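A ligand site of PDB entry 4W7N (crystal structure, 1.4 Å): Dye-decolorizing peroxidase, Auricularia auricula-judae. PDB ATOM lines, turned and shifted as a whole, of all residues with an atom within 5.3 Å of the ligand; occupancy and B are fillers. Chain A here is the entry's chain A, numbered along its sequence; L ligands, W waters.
The side-chain amide oxygen (OD1) of Asn 282 sits at hydrogen-bond distance from the guanidinium group (NH2) of Arg 256 (2.9 Å).
N of Leu 358 lies within hydrogen-bond range of O of Leu 220, at 2.9 Å.
The backbone carbonyl oxygen of His 305 sits at hydrogen-bond distance from the side-chain hydroxyl of Thr 309, at 3.2 Å.
OE2 of Glu 163 lies within hydrogen-bond range of N of Phe 167, at 2.7 Å.
OD1 of Asn 282 is in hydrogen-bond range of NH2 of Arg 312 (2.7 Å).
The backbone carbonyl oxygen of Val 254 sits at hydrogen-bond distance from the backbone NH of His 305, at 3.4 Å.
The side-chain carboxylate (OE1) of Glu 163 sits at hydrogen-bond distance from the side-chain amide nitrogen (NE2) of Gln 222, 2.8 Å away.
O of Ile 399 sits at hydrogen-bond distance from NE2 of Gln 375, 3.0 Å away.
Water W4 lies within hydrogen-bond range of an oxygen (O1) of the ligand and the guanidinium group (NH2) of Arg 256.
Water W2 lies within hydrogen-bond range of O of Arg 310 (2.7 Å), OH of Tyr 286 (2.7 Å), O3 of the ligand (2.8 Å), NE of Arg 312 (2.8 Å) and O of Ile 306 (2.9 Å).
NH2 of Arg 333 is in salt-bridge range of O2 of the ligand (2.7 Å).
The guanidinium group (NE) of Arg 256 lies within salt-bridge range of an oxygen (O1) of the ligand, 3.2 Å away.
NH2 of Arg 312 is in salt-bridge range of O3 of the ligand.
The backbone NH (N) of Ile 171 is in hydrogen-bond range of an oxygen (O2) of the ligand (2.8 Å).
A ring nitrogen (NE2) of His 305 binds an iron atom (FE1) of the ligand.
The backbone NH (N) of Gly 170 lies within hydrogen-bond range of an oxygen (O2) of the ligand (3.3 Å).
The backbone NH (N) of Ala 172 is in hydrogen-bond range of an oxygen (O2) of the ligand, at 3.0 Å.
Glu 163 touches the ligand (OE1 to C17, 3.3 Å).
CB of Phe 167 touches C9 of the ligand, at 3.5 Å.
O of Leu 168 touches C11 of the ligand (3.4 Å).
Asp 169 touches the ligand (OD1 to C11, 3.7 Å).
CD1 of Leu 220 touches C18 of the ligand, 3.8 Å away.
Gln 222 touches the ligand (NE2 to C17, 3.5 Å).
Val 254 touches the ligand.
CG2 of Ile 306 touches C1 of the ligand, at 3.6 Å.
Thr 309 touches the ligand (OG1 to C28, 3.2 Å).
Arg 310 touches the ligand.
CG1 of Ile 331 touches C31 of the ligand (3.9 Å).
CD2 of Leu 358 touches C15 of the ligand, 3.7 Å away.
Phe 360 touches the ligand.
Phe 371 touches the ligand.
Leu 374 touches the ligand (CB to C26, 3.9 Å).
OE1 of Gln 375 touches C24 of the ligand, 3.7 Å away.
CG2 of Ile 398 touches C14 of the ligand, at 3.95 Å.
Ile 399 touches the ligand (CG2 to C3, 3.5 Å).
CG2 of Val 427 touches C19 of the ligand (3.9 Å).
Hydrophobic or aromatic side chains within 4 Å of the ligand: Phe 167, Ile 171, Ala 172, Leu 220, Val 254, His 305, Ile 306, Ile 331, Leu 358, Phe 360, Phe 371, Leu 374, Ile 398, Ile 399 and Val 427.
26 residues have an atom within 4 Å of the ligand: Glu 163, Phe 167, Leu 168, Asp 169, Gly 170, Ile 171, Ala 172, Leu 220, Gln 222, Val 254, Arg 256, His 305, Ile 306, Thr 309, Arg 310, Arg 312, Ile 331, Arg 333, Leu 358, Phe 360, Phe 371, Leu 374, Gln 375, Ile 398, Ile 399 and Val 427.
The nearest printed residue that does not touch the ligand is Phe 165 (4.1 Å).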
ATOM      1  N   GLU A 163       6.465  20.566  29.598  1.00  0.00           N
ATOM      2  CA  GLU A 163       7.452  19.515  29.723  1.00  0.00           C
ATOM      3  C   GLU A 163       7.376  18.905  31.136  1.00  0.00           C
ATOM      4  O   GLU A 163       6.551  19.320  31.951  1.00  0.00           O
ATOM      5  CB  GLU A 163       8.859  20.014  29.353  1.00  0.00           C
ATOM      6  CG  GLU A 163       9.291  21.270  30.041  1.00  0.00           C
ATOM      7  CD  GLU A 163       9.543  21.049  31.504  1.00  0.00           C
ATOM      8  OE1 GLU A 163      10.323  20.131  31.835  1.00  0.00           O
ATOM      9  OE2 GLU A 163       8.935  21.756  32.327  1.00  0.00           O
ATOM     10  N   PHE A 165       9.025  18.959  33.972  1.00  0.00           N
ATOM     11  CA  PHE A 165       9.132  19.793  35.179  1.00  0.00           C
ATOM     12  C   PHE A 165       7.876  20.637  35.407  1.00  0.00           C
ATOM     13  O   PHE A 165       7.731  21.238  36.466  1.00  0.00           O
ATOM     14  CB  PHE A 165      10.338  20.741  35.139  1.00  0.00           C
ATOM     15  CG  PHE A 165      11.685  20.073  35.228  1.00  0.00           C
ATOM     16  CD1 PHE A 165      11.900  18.984  36.047  1.00  0.00           C
ATOM     17  CD2 PHE A 165      12.747  20.570  34.496  1.00  0.00           C
ATOM     18  CE1 PHE A 165      13.138  18.395  36.126  1.00  0.00           C
ATOM     19  CE2 PHE A 165      14.005  19.976  34.568  1.00  0.00           C
ATOM     20  CZ  PHE A 165      14.189  18.887  35.381  1.00  0.00           C
ATOM     21  N   PHE A 167       6.654  23.118  32.998  1.00  0.00           N
ATOM     22  CA  PHE A 167       6.695  24.434  32.349  1.00  0.00           C
ATOM     23  C   PHE A 167       6.158  24.366  30.918  1.00  0.00           C
ATOM     24  O   PHE A 167       6.520  23.461  30.146  1.00  0.00           O
ATOM     25  CB  PHE A 167       8.135  24.984  32.330  1.00  0.00           C
ATOM     26  CG  PHE A 167       8.668  25.321  33.694  1.00  0.00           C
ATOM     27  CD1 PHE A 167       9.145  24.317  34.531  1.00  0.00           C
ATOM     28  CD2 PHE A 167       8.695  26.635  34.140  1.00  0.00           C
ATOM     29  CE1 PHE A 167       9.618  24.628  35.799  1.00  0.00           C
ATOM     30  CE2 PHE A 167       9.168  26.946  35.408  1.00  0.00           C
ATOM     31  CZ  PHE A 167       9.634  25.936  36.232  1.00  0.00           C
ATOM     32  N   LEU A 168       5.296  25.315  30.566  1.00  0.00           N
ATOM     33  CA  LEU A 168       4.785  25.418  29.203  1.00  0.00           C
ATOM     34  C   LEU A 168       5.968  25.556  28.251  1.00  0.00           C
ATOM     35  O   LEU A 168       6.869  26.370  28.464  1.00  0.00           O
ATOM     36  CB  LEU A 168       3.852  26.616  29.056  1.00  0.00           C
ATOM     37  CG  LEU A 168       3.171  26.782  27.700  1.00  0.00           C
ATOM     38  CD1 LEU A 168       2.281  25.580  27.375  1.00  0.00           C
ATOM     39  CD2 LEU A 168       2.362  28.078  27.671  1.00  0.00           C
ATOM     40  N   ASP A 169       5.959  24.758  27.199  1.00  0.00           N
ATOM     41  CA  ASP A 169       7.073  24.677  26.277  1.00  0.00           C
ATOM     42  C   ASP A 169       6.583  24.936  24.846  1.00  0.00           C
ATOM     43  O   ASP A 169       5.382  24.836  24.569  1.00  0.00           O
ATOM     44  CB  ASP A 169       7.735  23.303  26.402  1.00  0.00           C
ATOM     45  CG  ASP A 169       9.075  23.218  25.685  1.00  0.00           C
ATOM     46  OD1 ASP A 169       9.664  24.275  25.371  1.00  0.00           O
ATOM     47  OD2 ASP A 169       9.540  22.082  25.446  1.00  0.00           O
ATOM     48  N   GLY A 170       7.497  25.276  23.953  1.00  0.00           N
ATOM     49  CA  GLY A 170       7.147  25.493  22.563  1.00  0.00           C
ATOM     50  C   GLY A 170       6.647  26.901  22.278  1.00  0.00           C
ATOM     51  O   GLY A 170       6.046  27.152  21.236  1.00  0.00           O
ATOM     52  N   ILE A 171       6.884  27.811  23.202  1.00  0.00           N
ATOM     53  CA  ILE A 171       6.455  29.195  23.029  1.00  0.00           C
ATOM     54  C   ILE A 171       7.350  29.935  22.032  1.00  0.00           C
ATOM     55  O   ILE A 171       6.860  30.579  21.093  1.00  0.00           O
ATOM     56  CB  ILE A 171       6.514  29.944  24.370  1.00  0.00           C
ATOM     57  CG1 ILE A 171       5.533  29.319  25.357  1.00  0.00           C
ATOM     58  CG2 ILE A 171       6.217  31.419  24.173  1.00  0.00           C
ATOM     59  CD1 ILE A 171       5.709  29.822  26.780  1.00  0.00           C
ATOM     60  N   ALA A 172       8.660  29.823  22.229  1.00  0.00           N
ATOM     61  CA  ALA A 172       9.616  30.631  21.498  1.00  0.00           C
ATOM     62  C   ALA A 172      10.312  29.870  20.367  1.00  0.00           C
ATOM     63  O   ALA A 172      10.949  28.835  20.594  1.00  0.00           O
ATOM     64  CB  ALA A 172      10.635  31.199  22.470  1.00  0.00           C
ATOM     65  N   GLN A 173      10.182  30.398  19.162  1.00  0.00           N
ATOM     66  CA  GLN A 173      10.894  29.884  17.995  1.00  0.00           C
ATOM     67  C   GLN A 173      11.373  31.064  17.163  1.00  0.00           C
ATOM     68  O   GLN A 173      10.766  32.136  17.193  1.00  0.00           O
ATOM     69  CB  GLN A 173       9.961  29.022  17.133  1.00  0.00           C
ATOM     70  CG  GLN A 173       9.229  27.907  17.875  1.00  0.00           C
ATOM     71  CD  GLN A 173      10.074  26.677  18.114  1.00  0.00           C
ATOM     72  OE1 GLN A 173      11.296  26.700  17.974  1.00  0.00           O
ATOM     73  NE2 GLN A 173       9.413  25.596  18.504  1.00  0.00           N
ATOM     74  N   LEU A 220      17.101  13.332  27.060  1.00  0.00           N
ATOM     75  CA  LEU A 220      17.448  14.032  28.284  1.00  0.00           C
ATOM     76  C   LEU A 220      16.520  13.651  29.415  1.00  0.00           C
ATOM     77  O   LEU A 220      15.373  14.090  29.466  1.00  0.00           O
ATOM     78  CB  LEU A 220      17.405  15.550  28.057  1.00  0.00           C
ATOM     79  CG  LEU A 220      18.339  16.052  26.953  1.00  0.00           C
ATOM     80  CD1 LEU A 220      18.158  17.548  26.738  1.00  0.00           C
ATOM     81  CD2 LEU A 220      19.787  15.719  27.300  1.00  0.00           C
ATOM     82  N   GLN A 222      14.896  13.703  32.998  1.00  0.00           N
ATOM     83  CA  GLN A 222      14.639  14.750  33.971  1.00  0.00           C
ATOM     84  C   GLN A 222      14.298  14.119  35.322  1.00  0.00           C
ATOM     85  O   GLN A 222      13.464  13.216  35.406  1.00  0.00           O
ATOM     86  CB  GLN A 222      13.498  15.648  33.510  1.00  0.00           C
ATOM     87  CG  GLN A 222      13.817  16.399  32.233  1.00  0.00           C
ATOM     88  CD  GLN A 222      12.619  17.122  31.666  1.00  0.00           C
ATOM     89  OE1 GLN A 222      12.128  16.778  30.596  1.00  0.00           O
ATOM     90  NE2 GLN A 222      12.153  18.135  32.381  1.00  0.00           N
ATOM     91  N   VAL A 254      14.245  28.923  35.002  1.00  0.00           N
ATOM     92  CA  VAL A 254      13.863  28.735  33.613  1.00  0.00           C
ATOM     93  C   VAL A 254      13.834  30.044  32.838  1.00  0.00           C
ATOM     94  O   VAL A 254      14.218  30.094  31.665  1.00  0.00           O
ATOM     95  CB  VAL A 254      12.471  28.063  33.522  1.00  0.00           C
ATOM     96  CG1 VAL A 254      11.974  28.048  32.085  1.00  0.00           C
ATOM     97  CG2 VAL A 254      12.537  26.646  34.075  1.00  0.00           C
ATOM     98  N   ARG A 256      10.871  31.596  32.752  1.00  0.00           N
ATOM     99  CA  ARG A 256       9.424  31.715  32.632  1.00  0.00           C
ATOM    100  C   ARG A 256       8.790  30.998  33.804  1.00  0.00           C
ATOM    101  O   ARG A 256       9.340  30.005  34.297  1.00  0.00           O
ATOM    102  CB  ARG A 256       8.903  31.071  31.343  1.00  0.00           C
ATOM    103  CG  ARG A 256       9.357  31.709  30.045  1.00  0.00           C
ATOM    104  CD  ARG A 256       8.713  31.048  28.832  1.00  0.00           C
ATOM    105  NE  ARG A 256       9.182  31.667  27.607  1.00  0.00           N
ATOM    106  CZ  ARG A 256       8.651  32.759  27.069  1.00  0.00           C
ATOM    107  NH1 ARG A 256       7.591  33.342  27.616  1.00  0.00           N
ATOM    108  NH2 ARG A 256       9.175  33.274  25.962  1.00  0.00           N
ATOM    109  N   ASN A 282       6.268  36.917  24.502  1.00  0.00           N
ATOM    110  CA  ASN A 282       7.651  36.931  24.032  1.00  0.00           C
ATOM    111  C   ASN A 282       8.171  38.341  23.772  1.00  0.00           C
ATOM    112  O   ASN A 282       9.246  38.519  23.236  1.00  0.00           O
ATOM    113  CB  ASN A 282       7.811  36.078  22.769  1.00  0.00           C
ATOM    114  CG  ASN A 282       9.128  35.335  22.740  1.00  0.00           C
ATOM    115  OD1 ASN A 282       9.756  35.130  23.773  1.00  0.00           O
ATOM    116  ND2 ASN A 282       9.545  34.919  21.552  1.00  0.00           N
ATOM    117  N   TYR A 286      15.111  41.828  27.717  1.00  0.00           N
ATOM    118  CA  TYR A 286      15.922  41.803  28.951  1.00  0.00           C
ATOM    119  C   TYR A 286      16.409  43.177  29.378  1.00  0.00           C
ATOM    120  O   TYR A 286      16.939  43.333  30.471  1.00  0.00           O
ATOM    121  CB  TYR A 286      17.097  40.817  28.874  1.00  0.00           C
ATOM    122  CG  TYR A 286      16.631  39.378  28.750  1.00  0.00           C
ATOM    123  CD1 TYR A 286      15.725  38.851  29.661  1.00  0.00           C
ATOM    124  CD2 TYR A 286      17.066  38.576  27.709  1.00  0.00           C
ATOM    125  CE1 TYR A 286      15.282  37.543  29.539  1.00  0.00           C
ATOM    126  CE2 TYR A 286      16.636  37.274  27.590  1.00  0.00           C
ATOM    127  CZ  TYR A 286      15.745  36.762  28.505  1.00  0.00           C
ATOM    128  OH  TYR A 286      15.287  35.470  28.382  1.00  0.00           O
ATOM    129  N   HIS A 305      17.613  29.764  32.055  1.00  0.00           N
ATOM    130  CA  HIS A 305      17.703  28.928  30.874  1.00  0.00           C
ATOM    131  C   HIS A 305      17.431  29.681  29.559  1.00  0.00           C
ATOM    132  O   HIS A 305      18.238  29.604  28.632  1.00  0.00           O
ATOM    133  CB  HIS A 305      16.750  27.739  31.031  1.00  0.00           C
ATOM    134  CG  HIS A 305      16.714  26.838  29.838  1.00  0.00           C
ATOM    135  ND1 HIS A 305      17.838  26.255  29.292  1.00  0.00           N
ATOM    136  CD2 HIS A 305      15.669  26.407  29.085  1.00  0.00           C
ATOM    137  CE1 HIS A 305      17.494  25.517  28.259  1.00  0.00           C
ATOM    138  NE2 HIS A 305      16.183  25.587  28.117  1.00  0.00           N
ATOM    139  N   ILE A 306      16.317  30.397  29.448  1.00  0.00           N
ATOM    140  CA  ILE A 306      15.996  31.021  28.169  1.00  0.00           C
ATOM    141  C   ILE A 306      16.907  32.218  27.871  1.00  0.00           C
ATOM    142  O   ILE A 306      17.114  32.566  26.714  1.00  0.00           O
ATOM    143  CB  ILE A 306      14.518  31.443  28.022  1.00  0.00           C
ATOM    144  CG1 ILE A 306      14.108  32.455  29.096  1.00  0.00           C
ATOM    145  CG2 ILE A 306      13.628  30.210  28.083  1.00  0.00           C
ATOM    146  CD1 ILE A 306      12.877  33.241  28.696  1.00  0.00           C
ATOM    147  N   THR A 309      19.964  30.600  26.366  1.00  0.00           N
ATOM    148  CA  THR A 309      19.789  30.015  25.035  1.00  0.00           C
ATOM    149  C   THR A 309      19.334  31.023  23.977  1.00  0.00           C
ATOM    150  O   THR A 309      19.505  30.791  22.788  1.00  0.00           O
ATOM    151  CB  THR A 309      18.835  28.814  25.089  1.00  0.00           C
ATOM    152  OG1 THR A 309      17.554  29.247  25.555  1.00  0.00           O
ATOM    153  CG2 THR A 309      19.393  27.737  26.003  1.00  0.00           C
ATOM    154  N   ARG A 310      18.750  32.138  24.407  1.00  0.00           N
ATOM    155  CA  ARG A 310      18.556  33.295  23.530  1.00  0.00           C
ATOM    156  C   ARG A 310      18.806  34.566  24.329  1.00  0.00           C
ATOM    157  O   ARG A 310      17.889  35.107  24.970  1.00  0.00           O
ATOM    158  CB  ARG A 310      17.157  33.339  22.886  1.00  0.00           C
ATOM    159  CG  ARG A 310      17.043  34.502  21.902  1.00  0.00           C
ATOM    160  CD  ARG A 310      15.623  34.799  21.422  1.00  0.00           C
ATOM    161  NE  ARG A 310      15.589  36.080  20.693  1.00  0.00           N
ATOM    162  CZ  ARG A 310      14.504  36.806  20.476  1.00  0.00           C
ATOM    163  NH1 ARG A 310      13.321  36.394  20.909  1.00  0.00           N
ATOM    164  NH2 ARG A 310      14.596  37.958  19.825  1.00  0.00           N
ATOM    165  N   ARG A 312      19.262  37.683  23.618  1.00  0.00           N
ATOM    166  CA  ARG A 312      18.604  38.927  23.220  1.00  0.00           C
ATOM    167  C   ARG A 312      19.556  40.117  23.452  1.00  0.00           C
ATOM    168  O   ARG A 312      20.668  40.099  22.927  1.00  0.00           O
ATOM    169  CB  ARG A 312      17.268  39.093  23.948  1.00  0.00           C
ATOM    170  CG  ARG A 312      16.359  37.868  23.781  1.00  0.00           C
ATOM    171  CD  ARG A 312      14.908  38.064  24.266  1.00  0.00           C
ATOM    172  NE  ARG A 312      14.222  36.761  24.294  1.00  0.00           N
ATOM    173  CZ  ARG A 312      12.925  36.563  24.079  1.00  0.00           C
ATOM    174  NH1 ARG A 312      12.107  37.578  23.806  1.00  0.00           N
ATOM    175  NH2 ARG A 312      12.442  35.332  24.123  1.00  0.00           N
ATOM    176  N   ILE A 331      17.721  28.047  16.903  1.00  0.00           N
ATOM    177  CA  ILE A 331      17.305  26.688  16.615  1.00  0.00           C
ATOM    178  C   ILE A 331      15.780  26.595  16.617  1.00  0.00           C
ATOM    179  O   ILE A 331      15.113  27.315  17.358  1.00  0.00           O
ATOM    180  CB  ILE A 331      17.877  25.662  17.631  1.00  0.00           C
ATOM    181  CG1 ILE A 331      17.431  25.999  19.059  1.00  0.00           C
ATOM    182  CG2 ILE A 331      19.402  25.623  17.539  1.00  0.00           C
ATOM    183  CD1 ILE A 331      17.776  24.937  20.080  1.00  0.00           C
ATOM    184  N   ARG A 333      12.850  24.166  17.721  1.00  0.00           N
ATOM    185  CA  ARG A 333      12.709  23.051  18.654  1.00  0.00           C
ATOM    186  C   ARG A 333      11.408  22.279  18.434  1.00  0.00           C
ATOM    187  O   ARG A 333      10.332  22.870  18.354  1.00  0.00           O
ATOM    188  CB  ARG A 333      12.772  23.567  20.088  1.00  0.00           C
ATOM    189  CG  ARG A 333      14.141  24.137  20.469  1.00  0.00           C
ATOM    190  CD  ARG A 333      14.129  24.792  21.857  1.00  0.00           C
ATOM    191  NE  ARG A 333      13.124  25.859  21.904  1.00  0.00           N
ATOM    192  CZ  ARG A 333      12.122  25.935  22.775  1.00  0.00           C
ATOM    193  NH1 ARG A 333      11.944  25.030  23.729  1.00  0.00           N
ATOM    194  NH2 ARG A 333      11.265  26.939  22.677  1.00  0.00           N
ATOM    195  N   LEU A 358      12.758  14.566  28.357  1.00  0.00           N
ATOM    196  CA  LEU A 358      12.477  15.264  27.126  1.00  0.00           C
ATOM    197  C   LEU A 358      13.202  14.582  25.980  1.00  0.00           C
ATOM    198  O   LEU A 358      14.414  14.402  26.027  1.00  0.00           O
ATOM    199  CB  LEU A 358      12.933  16.722  27.219  1.00  0.00           C
ATOM    200  CG  LEU A 358      12.606  17.611  26.015  1.00  0.00           C
ATOM    201  CD1 LEU A 358      11.100  17.817  25.928  1.00  0.00           C
ATOM    202  CD2 LEU A 358      13.325  18.933  26.109  1.00  0.00           C
ATOM    203  N   PHE A 360      14.484  15.573  23.139  1.00  0.00           N
ATOM    204  CA  PHE A 360      14.878  16.888  22.638  1.00  0.00           C
ATOM    205  C   PHE A 360      15.246  16.799  21.156  1.00  0.00           C
ATOM    206  O   PHE A 360      16.006  15.924  20.739  1.00  0.00           O
ATOM    207  CB  PHE A 360      16.053  17.414  23.459  1.00  0.00           C
ATOM    208  CG  PHE A 360      16.630  18.696  22.936  1.00  0.00           C
ATOM    209  CD1 PHE A 360      16.147  19.918  23.368  1.00  0.00           C
ATOM    210  CD2 PHE A 360      17.662  18.677  21.996  1.00  0.00           C
ATOM    211  CE1 PHE A 360      16.685  21.107  22.897  1.00  0.00           C
ATOM    212  CE2 PHE A 360      18.197  19.856  21.524  1.00  0.00           C
ATOM    213  CZ  PHE A 360      17.700  21.071  21.962  1.00  0.00           C
ATOM    214  N   PHE A 371      22.570  23.984  18.237  1.00  0.00           N
ATOM    215  CA  PHE A 371      22.592  23.179  19.457  1.00  0.00           C
ATOM    216  C   PHE A 371      23.964  23.128  20.125  1.00  0.00           C
ATOM    217  O   PHE A 371      24.087  23.326  21.333  1.00  0.00           O
ATOM    218  CB  PHE A 371      22.142  21.730  19.191  1.00  0.00           C
ATOM    219  CG  PHE A 371      22.549  20.783  20.290  1.00  0.00           C
ATOM    220  CD1 PHE A 371      21.938  20.845  21.528  1.00  0.00           C
ATOM    221  CD2 PHE A 371      23.564  19.870  20.090  1.00  0.00           C
ATOM    222  CE1 PHE A 371      22.329  20.005  22.546  1.00  0.00           C
ATOM    223  CE2 PHE A 371      23.961  19.017  21.107  1.00  0.00           C
ATOM    224  CZ  PHE A 371      23.343  19.084  22.334  1.00  0.00           C
ATOM    225  N   LEU A 374      24.935  26.505  21.707  1.00  0.00           N
ATOM    226  CA  LEU A 374      24.124  26.850  22.864  1.00  0.00           C
ATOM    227  C   LEU A 374      24.508  26.006  24.075  1.00  0.00           C
ATOM    228  O   LEU A 374      24.528  26.496  25.210  1.00  0.00           O
ATOM    229  CB  LEU A 374      22.637  26.709  22.550  1.00  0.00           C
ATOM    230  CG  LEU A 374      22.140  27.673  21.457  1.00  0.00           C
ATOM    231  CD1 LEU A 374      20.703  27.378  21.090  1.00  0.00           C
ATOM    232  CD2 LEU A 374      22.304  29.130  21.876  1.00  0.00           C
ATOM    233  N   GLN A 375      24.814  24.726  23.849  1.00  0.00           N
ATOM    234  CA  GLN A 375      25.204  23.857  24.954  1.00  0.00           C
ATOM    235  C   GLN A 375      26.601  24.198  25.484  1.00  0.00           C
ATOM    236  O   GLN A 375      26.803  24.373  26.684  1.00  0.00           O
ATOM    237  CB  GLN A 375      25.154  22.388  24.524  1.00  0.00           C
ATOM    238  CG  GLN A 375      25.379  21.403  25.676  1.00  0.00           C
ATOM    239  CD  GLN A 375      24.212  21.351  26.653  1.00  0.00           C
ATOM    240  OE1 GLN A 375      23.072  21.104  26.265  1.00  0.00           O
ATOM    241  NE2 GLN A 375      24.504  21.569  27.926  1.00  0.00           N
ATOM    242  N   ILE A 398      19.166  24.462  34.234  1.00  0.00           N
ATOM    243  CA  ILE A 398      18.384  23.380  33.658  1.00  0.00           C
ATOM    244  C   ILE A 398      19.304  22.401  32.909  1.00  0.00           C
ATOM    245  O   ILE A 398      19.302  21.206  33.191  1.00  0.00           O
ATOM    246  CB  ILE A 398      17.259  23.923  32.742  1.00  0.00           C
ATOM    247  CG1 ILE A 398      16.381  24.932  33.493  1.00  0.00           C
ATOM    248  CG2 ILE A 398      16.410  22.782  32.197  1.00  0.00           C
ATOM    249  CD1 ILE A 398      15.823  24.438  34.821  1.00  0.00           C
ATOM    250  N   ILE A 399      20.091  22.908  31.963  1.00  0.00           N
ATOM    251  CA  ILE A 399      20.863  22.034  31.077  1.00  0.00           C
ATOM    252  C   ILE A 399      22.383  22.166  31.212  1.00  0.00           C
ATOM    253  O   ILE A 399      23.118  21.430  30.553  1.00  0.00           O
ATOM    254  CB  ILE A 399      20.500  22.264  29.584  1.00  0.00           C
ATOM    255  CG1 ILE A 399      20.755  23.703  29.166  1.00  0.00           C
ATOM    256  CG2 ILE A 399      19.041  21.889  29.335  1.00  0.00           C
ATOM    257  CD1 ILE A 399      20.833  23.905  27.648  1.00  0.00           C
ATOM    258  N   VAL A 427      18.870  17.354  34.978  1.00  0.00           N
ATOM    259  CA  VAL A 427      18.757  16.792  33.642  1.00  0.00           C
ATOM    260  C   VAL A 427      19.998  15.942  33.359  1.00  0.00           C
ATOM    261  O   VAL A 427      21.130  16.401  33.486  1.00  0.00           O
ATOM    262  CB  VAL A 427      18.650  17.906  32.570  1.00  0.00           C
ATOM    263  CG1 VAL A 427      18.661  17.307  31.169  1.00  0.00           C
ATOM    264  CG2 VAL A 427      17.387  18.724  32.783  1.00  0.00           C
HETATM  265  C1  LIG L   1      13.142  27.363  25.933  1.00  0.00           C
HETATM  266  C2  LIG L   1      12.820  23.544  28.925  1.00  0.00           C
HETATM  267  C3  LIG L   1      16.695  21.523  26.831  1.00  0.00           C
HETATM  268  C4  LIG L   1      17.291  25.503  24.106  1.00  0.00           C
HETATM  269  C5  LIG L   1      12.720  26.500  26.909  1.00  0.00           C
HETATM  270  C6  LIG L   1      11.580  26.704  27.782  1.00  0.00           C
HETATM  271  C7  LIG L   1      11.478  25.652  28.598  1.00  0.00           C
HETATM  272  C8  LIG L   1      12.574  24.745  28.291  1.00  0.00           C
HETATM  273  C9  LIG L   1      10.427  25.425  29.685  1.00  0.00           C
HETATM  274  C10 LIG L   1      10.630  27.929  27.748  1.00  0.00           C
HETATM  275  C11 LIG L   1       9.498  27.709  26.760  1.00  0.00           C
HETATM  276  C12 LIG L   1       9.764  28.458  25.473  1.00  0.00           C
HETATM  277  O1  LIG L   1      10.316  29.585  25.520  1.00  0.00           O
HETATM  278  O2  LIG L   1       9.409  27.922  24.403  1.00  0.00           O
HETATM  279  C13 LIG L   1      13.842  22.677  28.640  1.00  0.00           C
HETATM  280  C14 LIG L   1      14.095  21.415  29.299  1.00  0.00           C
HETATM  281  C15 LIG L   1      15.169  20.865  28.728  1.00  0.00           C
HETATM  282  C16 LIG L   1      15.608  21.740  27.664  1.00  0.00           C
HETATM  283  C17 LIG L   1      13.275  20.881  30.492  1.00  0.00           C
HETATM  284  C18 LIG L   1      15.867  19.524  29.059  1.00  0.00           C
HETATM  285  C19 LIG L   1      15.188  18.515  29.609  1.00  0.00           C
HETATM  286  C20 LIG L   1      17.243  22.455  25.959  1.00  0.00           C
HETATM  287  C21 LIG L   1      18.503  22.336  25.274  1.00  0.00           C
HETATM  288  C22 LIG L   1      18.669  23.441  24.519  1.00  0.00           C
HETATM  289  C23 LIG L   1      17.513  24.290  24.725  1.00  0.00           C
HETATM  290  C24 LIG L   1      19.461  21.135  25.395  1.00  0.00           C
HETATM  291  C25 LIG L   1      19.840  23.841  23.609  1.00  0.00           C
HETATM  292  C26 LIG L   1      21.078  23.360  23.795  1.00  0.00           C
HETATM  293  C27 LIG L   1      16.192  26.311  24.266  1.00  0.00           C
HETATM  294  C28 LIG L   1      15.909  27.492  23.468  1.00  0.00           C
HETATM  295  C29 LIG L   1      14.619  28.068  24.044  1.00  0.00           C
HETATM  296  C30 LIG L   1      14.250  27.187  25.130  1.00  0.00           C
HETATM  297  C31 LIG L   1      16.683  28.075  22.263  1.00  0.00           C
HETATM  298  C32 LIG L   1      13.875  29.336  23.551  1.00  0.00           C
HETATM  299  C33 LIG L   1      14.663  30.551  24.033  1.00  0.00           C
HETATM  300  C34 LIG L   1      14.090  31.836  23.503  1.00  0.00           C
HETATM  301  O3  LIG L   1      13.822  32.755  24.324  1.00  0.00           O
HETATM  302  O4  LIG L   1      13.889  31.956  22.261  1.00  0.00           O
HETATM  303  N1  LIG L   1      13.305  25.300  27.248  1.00  0.00           N
HETATM  304  N2  LIG L   1      14.762  22.835  27.632  1.00  0.00           N
HETATM  305  N3  LIG L   1      16.659  23.655  25.611  1.00  0.00           N
HETATM  306  N4  LIG L   1      15.199  26.174  25.233  1.00  0.00           N
HETATM  307 FE1  LIG L   1      15.095  24.585  26.572  1.00  0.00          FE
HETATM  308  O   HOH W   1      14.260  30.397  20.051  1.00  0.00           O
HETATM  309  O   HOH W   2      15.361  34.625  25.771  1.00  0.00           O
HETATM  310  O   HOH W   3      12.318  33.803  21.179  1.00  0.00           O
HETATM  311  O   HOH W   4      11.580  31.834  25.663  1.00  0.00           O
